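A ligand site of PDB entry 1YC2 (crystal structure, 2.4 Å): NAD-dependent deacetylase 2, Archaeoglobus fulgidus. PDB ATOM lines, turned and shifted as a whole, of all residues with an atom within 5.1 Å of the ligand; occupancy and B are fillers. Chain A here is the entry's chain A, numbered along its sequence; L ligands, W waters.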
ATOM      1  N   THR A  22     -10.818 -11.911 -30.561  1.00  0.00           N
ATOM      2  CA  THR A  22     -10.721 -11.741 -29.109  1.00  0.00           C
ATOM      3  C   THR A  22      -9.645 -12.585 -28.459  1.00  0.00           C
ATOM      4  O   THR A  22      -9.331 -13.675 -28.913  1.00  0.00           O
ATOM      5  CB  THR A  22     -12.061 -12.079 -28.431  1.00  0.00           C
ATOM      6  OG1 THR A  22     -12.329 -13.475 -28.555  1.00  0.00           O
ATOM      7  CG2 THR A  22     -13.200 -11.289 -29.087  1.00  0.00           C
ATOM      8  N   GLY A  23      -9.077 -12.048 -27.379  1.00  0.00           N
ATOM      9  CA  GLY A  23      -8.050 -12.755 -26.655  1.00  0.00           C
ATOM     10  C   GLY A  23      -8.461 -12.905 -25.209  1.00  0.00           C
ATOM     11  O   GLY A  23      -9.612 -12.654 -24.874  1.00  0.00           O
ATOM     12  N   ALA A  24      -7.514 -13.298 -24.352  1.00  0.00           N
ATOM     13  CA  ALA A  24      -7.782 -13.517 -22.936  1.00  0.00           C
ATOM     14  C   ALA A  24      -8.383 -12.310 -22.227  1.00  0.00           C
ATOM     15  O   ALA A  24      -9.111 -12.455 -21.249  1.00  0.00           O
ATOM     16  CB  ALA A  24      -6.495 -13.946 -22.211  1.00  0.00           C
ATOM     17  N   GLY A  25      -8.074 -11.115 -22.730  1.00  0.00           N
ATOM     18  CA  GLY A  25      -8.595  -9.909 -22.107  1.00  0.00           C
ATOM     19  C   GLY A  25     -10.113  -9.807 -22.083  1.00  0.00           C
ATOM     20  O   GLY A  25     -10.674  -9.147 -21.216  1.00  0.00           O
ATOM     21  N   ILE A  26     -10.798 -10.436 -23.034  1.00  0.00           N
ATOM     22  CA  ILE A  26     -12.255 -10.326 -23.042  1.00  0.00           C
ATOM     23  C   ILE A  26     -12.927 -11.240 -22.034  1.00  0.00           C
ATOM     24  O   ILE A  26     -14.130 -11.175 -21.839  1.00  0.00           O
ATOM     25  CB  ILE A  26     -12.862 -10.609 -24.430  1.00  0.00           C
ATOM     26  CG1 ILE A  26     -14.293 -10.038 -24.478  1.00  0.00           C
ATOM     27  CG2 ILE A  26     -12.914 -12.117 -24.700  1.00  0.00           C
ATOM     28  CD1 ILE A  26     -15.000 -10.180 -25.800  1.00  0.00           C
ATOM     29  N   ALA A  28     -11.418 -11.646 -18.842  1.00  0.00           N
ATOM     30  CA  ALA A  28     -10.904 -11.255 -17.535  1.00  0.00           C
ATOM     31  C   ALA A  28     -12.067 -10.906 -16.610  1.00  0.00           C
ATOM     32  O   ALA A  28     -12.131 -11.357 -15.472  1.00  0.00           O
ATOM     33  CB  ALA A  28      -9.950 -10.062 -17.676  1.00  0.00           C
ATOM     34  N   GLU A  29     -13.007 -10.107 -17.120  1.00  0.00           N
ATOM     35  CA  GLU A  29     -14.174  -9.698 -16.341  1.00  0.00           C
ATOM     36  C   GLU A  29     -15.168 -10.846 -16.143  1.00  0.00           C
ATOM     37  O   GLU A  29     -16.282 -10.626 -15.673  1.00  0.00           O
ATOM     38  CB  GLU A  29     -14.872  -8.518 -17.007  1.00  0.00           C
ATOM     39  CG  GLU A  29     -14.004  -7.289 -17.117  1.00  0.00           C
ATOM     40  CD  GLU A  29     -14.605  -6.221 -18.009  1.00  0.00           C
ATOM     41  OE1 GLU A  29     -15.644  -5.638 -17.628  1.00  0.00           O
ATOM     42  OE2 GLU A  29     -14.043  -5.984 -19.106  1.00  0.00           O
ATOM     43  N   THR A  34      -5.684 -13.469 -17.326  1.00  0.00           N
ATOM     44  CA  THR A  34      -5.002 -13.356 -18.616  1.00  0.00           C
ATOM     45  C   THR A  34      -3.640 -14.050 -18.605  1.00  0.00           C
ATOM     46  O   THR A  34      -3.253 -14.683 -17.620  1.00  0.00           O
ATOM     47  CB  THR A  34      -4.806 -11.879 -18.958  1.00  0.00           C
ATOM     48  OG1 THR A  34      -5.961 -11.146 -18.550  1.00  0.00           O
ATOM     49  CG2 THR A  34      -4.646 -11.706 -20.435  1.00  0.00           C
ATOM     50  N   PHE A  35      -2.905 -13.929 -19.718  1.00  0.00           N
ATOM     51  CA  PHE A  35      -1.576 -14.530 -19.857  1.00  0.00           C
ATOM     52  C   PHE A  35      -0.457 -13.759 -19.179  1.00  0.00           C
ATOM     53  O   PHE A  35       0.715 -13.966 -19.483  1.00  0.00           O
ATOM     54  CB  PHE A  35      -1.236 -14.703 -21.340  1.00  0.00           C
ATOM     55  CG  PHE A  35      -1.738 -15.984 -21.936  1.00  0.00           C
ATOM     56  CD1 PHE A  35      -1.037 -17.170 -21.735  1.00  0.00           C
ATOM     57  CD2 PHE A  35      -2.900 -15.999 -22.704  1.00  0.00           C
ATOM     58  CE1 PHE A  35      -1.498 -18.371 -22.283  1.00  0.00           C
ATOM     59  CE2 PHE A  35      -3.368 -17.196 -23.264  1.00  0.00           C
ATOM     60  CZ  PHE A  35      -2.660 -18.386 -23.051  1.00  0.00           C
ATOM     61  N   ARG A  36      -0.817 -12.863 -18.258  1.00  0.00           N
ATOM     62  CA  ARG A  36       0.175 -12.057 -17.547  1.00  0.00           C
ATOM     63  C   ARG A  36       1.207 -12.935 -16.832  1.00  0.00           C
ATOM     64  O   ARG A  36       0.861 -13.967 -16.254  1.00  0.00           O
ATOM     65  CB  ARG A  36      -0.512 -11.149 -16.514  1.00  0.00           C
ATOM     66  CG  ARG A  36      -0.088  -9.688 -16.586  1.00  0.00           C
ATOM     67  CD  ARG A  36      -0.879  -8.940 -17.646  1.00  0.00           C
ATOM     68  NE  ARG A  36      -2.308  -8.909 -17.330  1.00  0.00           N
ATOM     69  CZ  ARG A  36      -3.233  -8.281 -18.059  1.00  0.00           C
ATOM     70  NH1 ARG A  36      -4.508  -8.310 -17.686  1.00  0.00           N
ATOM     71  NH2 ARG A  36      -2.883  -7.616 -19.150  1.00  0.00           N
ATOM     72  N   GLU A  38       3.663 -14.831 -18.085  1.00  0.00           N
ATOM     73  CA  GLU A  38       3.869 -16.148 -18.701  1.00  0.00           C
ATOM     74  C   GLU A  38       5.346 -16.536 -18.611  1.00  0.00           C
ATOM     75  O   GLU A  38       5.677 -17.720 -18.556  1.00  0.00           O
ATOM     76  CB  GLU A  38       3.425 -16.124 -20.163  1.00  0.00           C
ATOM     77  CG  GLU A  38       3.776 -17.396 -20.930  1.00  0.00           C
ATOM     78  CD  GLU A  38       3.512 -17.275 -22.426  1.00  0.00           C
ATOM     79  OE1 GLU A  38       3.931 -18.190 -23.177  1.00  0.00           O
ATOM     80  OE2 GLU A  38       2.876 -16.288 -22.839  1.00  0.00           O
ATOM     81  N   GLN A 100      -8.990 -16.768 -29.530  1.00  0.00           N
ATOM     82  CA  GLN A 100      -7.837 -17.583 -29.143  1.00  0.00           C
ATOM     83  C   GLN A 100      -8.153 -18.264 -27.818  1.00  0.00           C
ATOM     84  O   GLN A 100      -7.384 -19.106 -27.358  1.00  0.00           O
ATOM     85  CB  GLN A 100      -6.581 -16.730 -28.989  1.00  0.00           C
ATOM     86  CG  GLN A 100      -5.830 -16.533 -30.284  1.00  0.00           C
ATOM     87  CD  GLN A 100      -4.466 -15.906 -30.109  1.00  0.00           C
ATOM     88  OE1 GLN A 100      -3.710 -15.753 -31.077  1.00  0.00           O
ATOM     89  NE2 GLN A 100      -4.140 -15.516 -28.879  1.00  0.00           N
ATOM     90  N   ASN A 101      -9.272 -17.892 -27.218  1.00  0.00           N
ATOM     91  CA  ASN A 101      -9.678 -18.466 -25.940  1.00  0.00           C
ATOM     92  C   ASN A 101     -10.246 -19.875 -26.128  1.00  0.00           C
ATOM     93  O   ASN A 101     -10.755 -20.219 -27.189  1.00  0.00           O
ATOM     94  CB  ASN A 101     -10.739 -17.581 -25.280  1.00  0.00           C
ATOM     95  CG  ASN A 101     -10.255 -16.167 -25.074  1.00  0.00           C
ATOM     96  OD1 ASN A 101      -9.061 -15.913 -24.985  1.00  0.00           O
ATOM     97  ND2 ASN A 101     -11.201 -15.226 -24.980  1.00  0.00           N
ATOM     98  N   HIS A 118      -7.251 -21.952 -31.031  1.00  0.00           N
ATOM     99  CA  HIS A 118      -6.501 -22.843 -30.155  1.00  0.00           C
ATOM    100  C   HIS A 118      -7.343 -24.007 -29.660  1.00  0.00           C
ATOM    101  O   HIS A 118      -6.971 -24.672 -28.705  1.00  0.00           O
ATOM    102  CB  HIS A 118      -5.934 -22.076 -28.953  1.00  0.00           C
ATOM    103  CG  HIS A 118      -4.887 -21.065 -29.300  1.00  0.00           C
ATOM    104  ND1 HIS A 118      -4.202 -21.093 -30.494  1.00  0.00           N
ATOM    105  CD2 HIS A 118      -4.385 -20.026 -28.601  1.00  0.00           C
ATOM    106  CE1 HIS A 118      -3.313 -20.101 -30.514  1.00  0.00           C
ATOM    107  NE2 HIS A 118      -3.405 -19.443 -29.378  1.00  0.00           N
ATOM    108  N   GLY A 191      -9.387  -7.367 -26.325  1.00  0.00           N
ATOM    109  CA  GLY A 191      -8.648  -8.149 -25.350  1.00  0.00           C
ATOM    110  C   GLY A 191      -7.542  -9.063 -25.852  1.00  0.00           C
ATOM    111  O   GLY A 191      -7.438 -10.213 -25.416  1.00  0.00           O
ATOM    112  N   SER A 192      -6.708  -8.551 -26.746  1.00  0.00           N
ATOM    113  CA  SER A 192      -5.594  -9.324 -27.270  1.00  0.00           C
ATOM    114  C   SER A 192      -4.366  -8.441 -27.368  1.00  0.00           C
ATOM    115  O   SER A 192      -4.450  -7.316 -27.846  1.00  0.00           O
ATOM    116  CB  SER A 192      -5.929  -9.890 -28.648  1.00  0.00           C
ATOM    117  OG  SER A 192      -4.802 -10.582 -29.156  1.00  0.00           O
ATOM    118  N   SER A 193      -3.220  -8.940 -26.928  1.00  0.00           N
ATOM    119  CA  SER A 193      -2.001  -8.165 -26.991  1.00  0.00           C
ATOM    120  C   SER A 193      -1.414  -8.175 -28.410  1.00  0.00           C
ATOM    121  O   SER A 193      -0.440  -7.464 -28.700  1.00  0.00           O
ATOM    122  CB  SER A 193      -0.972  -8.719 -26.004  1.00  0.00           C
ATOM    123  OG  SER A 193      -0.534 -10.014 -26.383  1.00  0.00           O
ATOM    124  N   LEU A 194      -2.011  -8.989 -29.289  1.00  0.00           N
ATOM    125  CA  LEU A 194      -1.597  -9.091 -30.685  1.00  0.00           C
ATOM    126  C   LEU A 194      -0.083  -9.301 -30.842  1.00  0.00           C
ATOM    127  O   LEU A 194       0.529  -8.734 -31.738  1.00  0.00           O
ATOM    128  CB  LEU A 194      -2.006  -7.833 -31.444  1.00  0.00           C
ATOM    129  CG  LEU A 194      -3.487  -7.447 -31.349  1.00  0.00           C
ATOM    130  CD1 LEU A 194      -3.750  -6.194 -32.169  1.00  0.00           C
ATOM    131  CD2 LEU A 194      -4.335  -8.610 -31.850  1.00  0.00           C
ATOM    132  N   VAL A 195       0.487 -10.134 -29.988  1.00  0.00           N
ATOM    133  CA  VAL A 195       1.931 -10.365 -30.020  1.00  0.00           C
ATOM    134  C   VAL A 195       2.420 -11.557 -30.825  1.00  0.00           C
ATOM    135  O   VAL A 195       3.490 -11.502 -31.417  1.00  0.00           O
ATOM    136  CB  VAL A 195       2.477 -10.468 -28.563  1.00  0.00           C
ATOM    137  CG1 VAL A 195       3.942 -10.896 -28.572  1.00  0.00           C
ATOM    138  CG2 VAL A 195       2.317  -9.121 -27.866  1.00  0.00           C
ATOM    139  N   VAL A 196       1.637 -12.629 -30.868  1.00  0.00           N
ATOM    140  CA  VAL A 196       2.060 -13.828 -31.583  1.00  0.00           C
ATOM    141  C   VAL A 196       1.085 -14.282 -32.675  1.00  0.00           C
ATOM    142  O   VAL A 196      -0.125 -14.123 -32.556  1.00  0.00           O
ATOM    143  CB  VAL A 196       2.252 -15.000 -30.586  1.00  0.00           C
ATOM    144  CG1 VAL A 196       2.663 -16.264 -31.310  1.00  0.00           C
ATOM    145  CG2 VAL A 196       3.298 -14.623 -29.549  1.00  0.00           C
ATOM    146  N   VAL A 216     -10.130  -2.505 -28.860  1.00  0.00           N
ATOM    147  CA  VAL A 216     -10.532  -2.192 -27.505  1.00  0.00           C
ATOM    148  C   VAL A 216      -9.648  -3.074 -26.649  1.00  0.00           C
ATOM    149  O   VAL A 216      -9.806  -4.299 -26.625  1.00  0.00           O
ATOM    150  CB  VAL A 216     -12.007  -2.576 -27.244  1.00  0.00           C
ATOM    151  CG1 VAL A 216     -12.345  -2.308 -25.780  1.00  0.00           C
ATOM    152  CG2 VAL A 216     -12.941  -1.802 -28.173  1.00  0.00           C
ATOM    153  N   ASN A 217      -8.694  -2.463 -25.964  1.00  0.00           N
ATOM    154  CA  ASN A 217      -7.795  -3.224 -25.142  1.00  0.00           C
ATOM    155  C   ASN A 217      -7.438  -2.433 -23.898  1.00  0.00           C
ATOM    156  O   ASN A 217      -7.499  -1.211 -23.903  1.00  0.00           O
ATOM    157  CB  ASN A 217      -6.539  -3.560 -25.945  1.00  0.00           C
ATOM    158  CG  ASN A 217      -5.907  -4.835 -25.501  1.00  0.00           C
ATOM    159  OD1 ASN A 217      -6.553  -5.885 -25.486  1.00  0.00           O
ATOM    160  ND2 ASN A 217      -4.627  -4.769 -25.137  1.00  0.00           N
ATOM    161  N   ALA A 218      -7.066  -3.132 -22.828  1.00  0.00           N
ATOM    162  CA  ALA A 218      -6.705  -2.480 -21.580  1.00  0.00           C
ATOM    163  C   ALA A 218      -5.367  -1.760 -21.705  1.00  0.00           C
ATOM    164  O   ALA A 218      -5.110  -0.790 -20.995  1.00  0.00           O
ATOM    165  CB  ALA A 218      -6.645  -3.495 -20.451  1.00  0.00           C
ATOM    166  N   GLU A 219      -4.538  -2.250 -22.613  1.00  0.00           N
ATOM    167  CA  GLU A 219      -3.222  -1.676 -22.837  1.00  0.00           C
ATOM    168  C   GLU A 219      -2.927  -1.543 -24.318  1.00  0.00           C
ATOM    169  O   GLU A 219      -3.466  -2.294 -25.139  1.00  0.00           O
ATOM    170  CB  GLU A 219      -2.146  -2.543 -22.205  1.00  0.00           C
ATOM    171  CG  GLU A 219      -2.353  -2.795 -20.736  1.00  0.00           C
ATOM    172  CD  GLU A 219      -1.163  -3.500 -20.119  1.00  0.00           C
ATOM    173  OE1 GLU A 219      -0.789  -4.573 -20.628  1.00  0.00           O
ATOM    174  OE2 GLU A 219      -0.614  -2.967 -19.120  1.00  0.00           O
ATOM    175  N   THR A 221      -0.868  -1.765 -27.913  1.00  0.00           N
ATOM    176  CA  THR A 221      -0.096  -2.833 -28.531  1.00  0.00           C
ATOM    177  C   THR A 221       0.721  -2.203 -29.650  1.00  0.00           C
ATOM    178  O   THR A 221       0.479  -1.067 -30.037  1.00  0.00           O
ATOM    179  CB  THR A 221      -1.016  -3.922 -29.134  1.00  0.00           C
ATOM    180  OG1 THR A 221      -1.672  -3.412 -30.307  1.00  0.00           O
ATOM    181  CG2 THR A 221      -2.088  -4.332 -28.127  1.00  0.00           C
ATOM    182  N   GLY A 233      -9.512   0.571 -22.143  1.00  0.00           N
ATOM    183  CA  GLY A 233     -10.479   0.329 -21.087  1.00  0.00           C
ATOM    184  C   GLY A 233     -10.868  -1.135 -21.005  1.00  0.00           C
ATOM    185  O   GLY A 233     -10.276  -1.976 -21.676  1.00  0.00           O
ATOM    186  N   LYS A 234     -11.875  -1.447 -20.188  1.00  0.00           N
ATOM    187  CA  LYS A 234     -12.325  -2.823 -20.034  1.00  0.00           C
ATOM    188  C   LYS A 234     -13.405  -3.198 -21.047  1.00  0.00           C
ATOM    189  O   LYS A 234     -14.336  -2.425 -21.298  1.00  0.00           O
ATOM    190  CB  LYS A 234     -12.841  -3.052 -18.610  1.00  0.00           C
ATOM    191  CG  LYS A 234     -11.766  -2.909 -17.552  1.00  0.00           C
ATOM    192  CD  LYS A 234     -12.318  -3.150 -16.161  1.00  0.00           C
ATOM    193  CE  LYS A 234     -11.199  -3.094 -15.133  1.00  0.00           C
ATOM    194  NZ  LYS A 234     -11.680  -3.390 -13.761  1.00  0.00           N
ATOM    195  N   ALA A 235     -13.264  -4.385 -21.618  1.00  0.00           N
ATOM    196  CA  ALA A 235     -14.205  -4.875 -22.621  1.00  0.00           C
ATOM    197  C   ALA A 235     -15.632  -4.970 -22.092  1.00  0.00           C
ATOM    198  O   ALA A 235     -16.569  -4.562 -22.774  1.00  0.00           O
ATOM    199  CB  ALA A 235     -13.757  -6.237 -23.126  1.00  0.00           C
ATOM    200  N   GLY A 236     -15.774  -5.500 -20.885  1.00  0.00           N
ATOM    201  CA  GLY A 236     -17.089  -5.649 -20.284  1.00  0.00           C
ATOM    202  C   GLY A 236     -17.802  -4.321 -20.124  1.00  0.00           C
ATOM    203  O   GLY A 236     -19.024  -4.276 -20.017  1.00  0.00           O
HETATM  204  P1  LIG L   1      -2.605 -11.859 -23.804  1.00  0.00           P
HETATM  205  O1  LIG L   1      -1.292 -11.771 -24.484  1.00  0.00           O
HETATM  206  O2  LIG L   1      -2.654 -12.204 -22.349  1.00  0.00           O
HETATM  207  O3  LIG L   1      -3.346 -10.473 -24.097  1.00  0.00           O
HETATM  208  C1  LIG L   1      -4.605 -10.074 -23.458  1.00  0.00           C
HETATM  209  C2  LIG L   1      -4.740  -8.560 -23.611  1.00  0.00           C
HETATM  210  O4  LIG L   1      -6.018  -8.209 -22.951  1.00  0.00           O
HETATM  211  C3  LIG L   1      -3.658  -7.682 -22.890  1.00  0.00           C
HETATM  212  O5  LIG L   1      -2.981  -6.850 -23.880  1.00  0.00           O
HETATM  213  C4  LIG L   1      -4.389  -6.863 -21.825  1.00  0.00           C
HETATM  214  O6  LIG L   1      -3.919  -5.588 -21.557  1.00  0.00           O
HETATM  215  C5  LIG L   1      -5.847  -6.934 -22.329  1.00  0.00           C
HETATM  216  N1  LIG L   1      -6.836  -6.900 -21.245  1.00  0.00           N
HETATM  217  C6  LIG L   1      -6.798  -7.289 -19.908  1.00  0.00           C
HETATM  218  N2  LIG L   1      -7.938  -7.091 -19.281  1.00  0.00           N
HETATM  219  C7  LIG L   1      -8.812  -6.568 -20.163  1.00  0.00           C
HETATM  220  C8  LIG L   1     -10.231  -6.143 -20.070  1.00  0.00           C
HETATM  221  N3  LIG L   1     -10.931  -6.226 -18.957  1.00  0.00           N
HETATM  222  N4  LIG L   1     -10.766  -5.635 -21.239  1.00  0.00           N
HETATM  223  C9  LIG L   1     -10.105  -5.521 -22.412  1.00  0.00           C
HETATM  224  N5  LIG L   1      -8.762  -5.912 -22.557  1.00  0.00           N
HETATM  225  C10 LIG L   1      -8.156  -6.435 -21.399  1.00  0.00           C
HETATM  226  O7  LIG L   1      -3.520 -12.907 -24.550  1.00  0.00           O
HETATM  227  P2  LIG L   1      -3.870 -13.115 -26.111  1.00  0.00           P
HETATM  228  O8  LIG L   1      -3.808 -11.815 -26.796  1.00  0.00           O
HETATM  229  O9  LIG L   1      -5.143 -13.908 -26.127  1.00  0.00           O
HETATM  230  O10 LIG L   1      -2.593 -13.985 -26.579  1.00  0.00           O
HETATM  231  C11 LIG L   1      -2.414 -15.324 -26.037  1.00  0.00           C
HETATM  232  C12 LIG L   1      -1.309 -16.048 -26.708  1.00  0.00           C
HETATM  233  O11 LIG L   1      -0.145 -15.128 -26.910  1.00  0.00           O
HETATM  234  C13 LIG L   1      -0.743 -17.240 -25.879  1.00  0.00           C
HETATM  235  O12 LIG L   1      -0.464 -18.374 -26.739  1.00  0.00           O
HETATM  236  C14 LIG L   1       0.544 -16.679 -25.233  1.00  0.00           C
HETATM  237  O13 LIG L   1       1.460 -17.679 -24.872  1.00  0.00           O
HETATM  238  C15 LIG L   1       1.074 -15.677 -26.333  1.00  0.00           C
HETATM  239  N6  LIG L   1       1.903 -14.530 -25.797  1.00  0.00           N
HETATM  240  C16 LIG L   1       3.343 -14.736 -25.770  1.00  0.00           C
HETATM  241  C17 LIG L   1       4.180 -13.783 -25.338  1.00  0.00           C
HETATM  242  C18 LIG L   1       5.691 -14.011 -25.298  1.00  0.00           C
HETATM  243  O14 LIG L   1       6.436 -13.001 -25.217  1.00  0.00           O
HETATM  244  N7  LIG L   1       6.176 -15.268 -25.337  1.00  0.00           N
HETATM  245  C19 LIG L   1       3.633 -12.455 -24.857  1.00  0.00           C
HETATM  246  C20 LIG L   1       2.151 -12.235 -24.876  1.00  0.00           C
HETATM  247  C21 LIG L   1       1.322 -13.287 -25.354  1.00  0.00           C
HETATM  248  O   HOH W   1      -0.877 -12.458 -28.721  1.00  0.00           O
HETATM  249  O   HOH W   2      -6.467 -16.235 -25.285  1.00  0.00           O
HETATM  250  O   HOH W   3      -1.768  -9.890 -20.769  1.00  0.00           O
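The backbone NH (N) of Ser 193 lies within hydrogen-bond range of an oxygen (O8) of the ligand.
OG of Ser 193 lies within hydrogen-bond range of O1 of the ligand (2.7 Å).
N4 of the ligand is in hydrogen-bond range of N of Ala 235.
OE2 of Glu 38 is in hydrogen-bond range of O13 of the ligand.
The side-chain hydroxyl (OG) of Ser 192 is in hydrogen-bond range of an oxygen (O8) of the ligand (2.8 Å).
An oxygen (O5) of the ligand is in hydrogen-bond range of the side-chain amide nitrogen (ND2) of Asn 217 (2.9 Å).
N of Ala 24 lies within hydrogen-bond range of O9 of the ligand (3.0 Å).
O2 of the ligand sits close to N of Phe 35, 3.2 Å away.
N3 of the ligand lies within hydrogen-bond range of OE2 of Glu 29.
An oxygen (O6) of the ligand lies close to the guanidinium group (NH2) of Arg 36 (3.3 Å).
O10 of the ligand is in hydrogen-bond range of NE2 of Gln 100 (3.2 Å).
The backbone NH (N) of Ala 218 is in hydrogen-bond range of a nitrogen (N5) of the ligand, at 3.3 Å.
OE1 of Glu 219 sits close to O6 of the ligand.
The backbone NH (N) of Ala 235 sits at hydrogen-bond distance from the side-chain carboxylate (OE2) of Glu 29.
N of Ser 192 sits at hydrogen-bond distance from OD1 of Asn 217, 3.0 Å away.
OD1 of Asn 217 sits close to N of Gly 191, at 3.3 Å.
The backbone carbonyl oxygen (O) of Gly 191 sits at hydrogen-bond distance from the backbone NH (N) of Ala 24 (3.3 Å).
The guanidinium group (NH2) of Arg 36 lies within salt-bridge range of the side-chain carboxylate (OE1) of Glu 219 (3.98 Å).
The backbone NH (N) of Gln 100 sits at hydrogen-bond distance from the backbone carbonyl oxygen (O) of Thr 22 (3.2 Å).
The backbone NH (N) of Gly 25 sits at hydrogen-bond distance from the backbone carbonyl oxygen (O) of Gly 191, 2.9 Å away.
The backbone NH of Gly 191 lies within hydrogen-bond range of the backbone carbonyl oxygen of Val 216 (3.1 Å).
An oxygen (O4) of the ligand sits close to the backbone carbonyl oxygen (O) of Gly 191, at 3.5 Å.
Merely in contact with the ligand: Gly 23, Gly 25, Ala 28, Thr 34, Val 196, Gly 233 and Lys 234.
20 residues have an atom within 4 Å of the ligand: Gly 23, Ala 24, Gly 25, Ala 28, Glu 29, Thr 34, Phe 35, Arg 36, Glu 38, Gln 100, Gly 191, Ser 192, Ser 193, Val 196, Asn 217, Ala 218, Glu 219, Gly 233, Lys 234 and Ala 235.
The nearest printed residue that does not touch the ligand is Val 195 (4.04 Å).
Water W2 lies within hydrogen-bond range of OD1 of Asn 101, O9 of the ligand and N of Ala 24.
Water W3 lies within hydrogen-bond range of an oxygen (O2) of the ligand (2.9 Å) and the guanidinium group (NH2) of Arg 36 (3.0 Å).
Water W1 lies within hydrogen-bond range of N of Val 195 (3.0 Å), O10 of the ligand (3.1 Å), N of Val 196 (3.3 Å) and OG of Ser 193 (3.4 Å).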
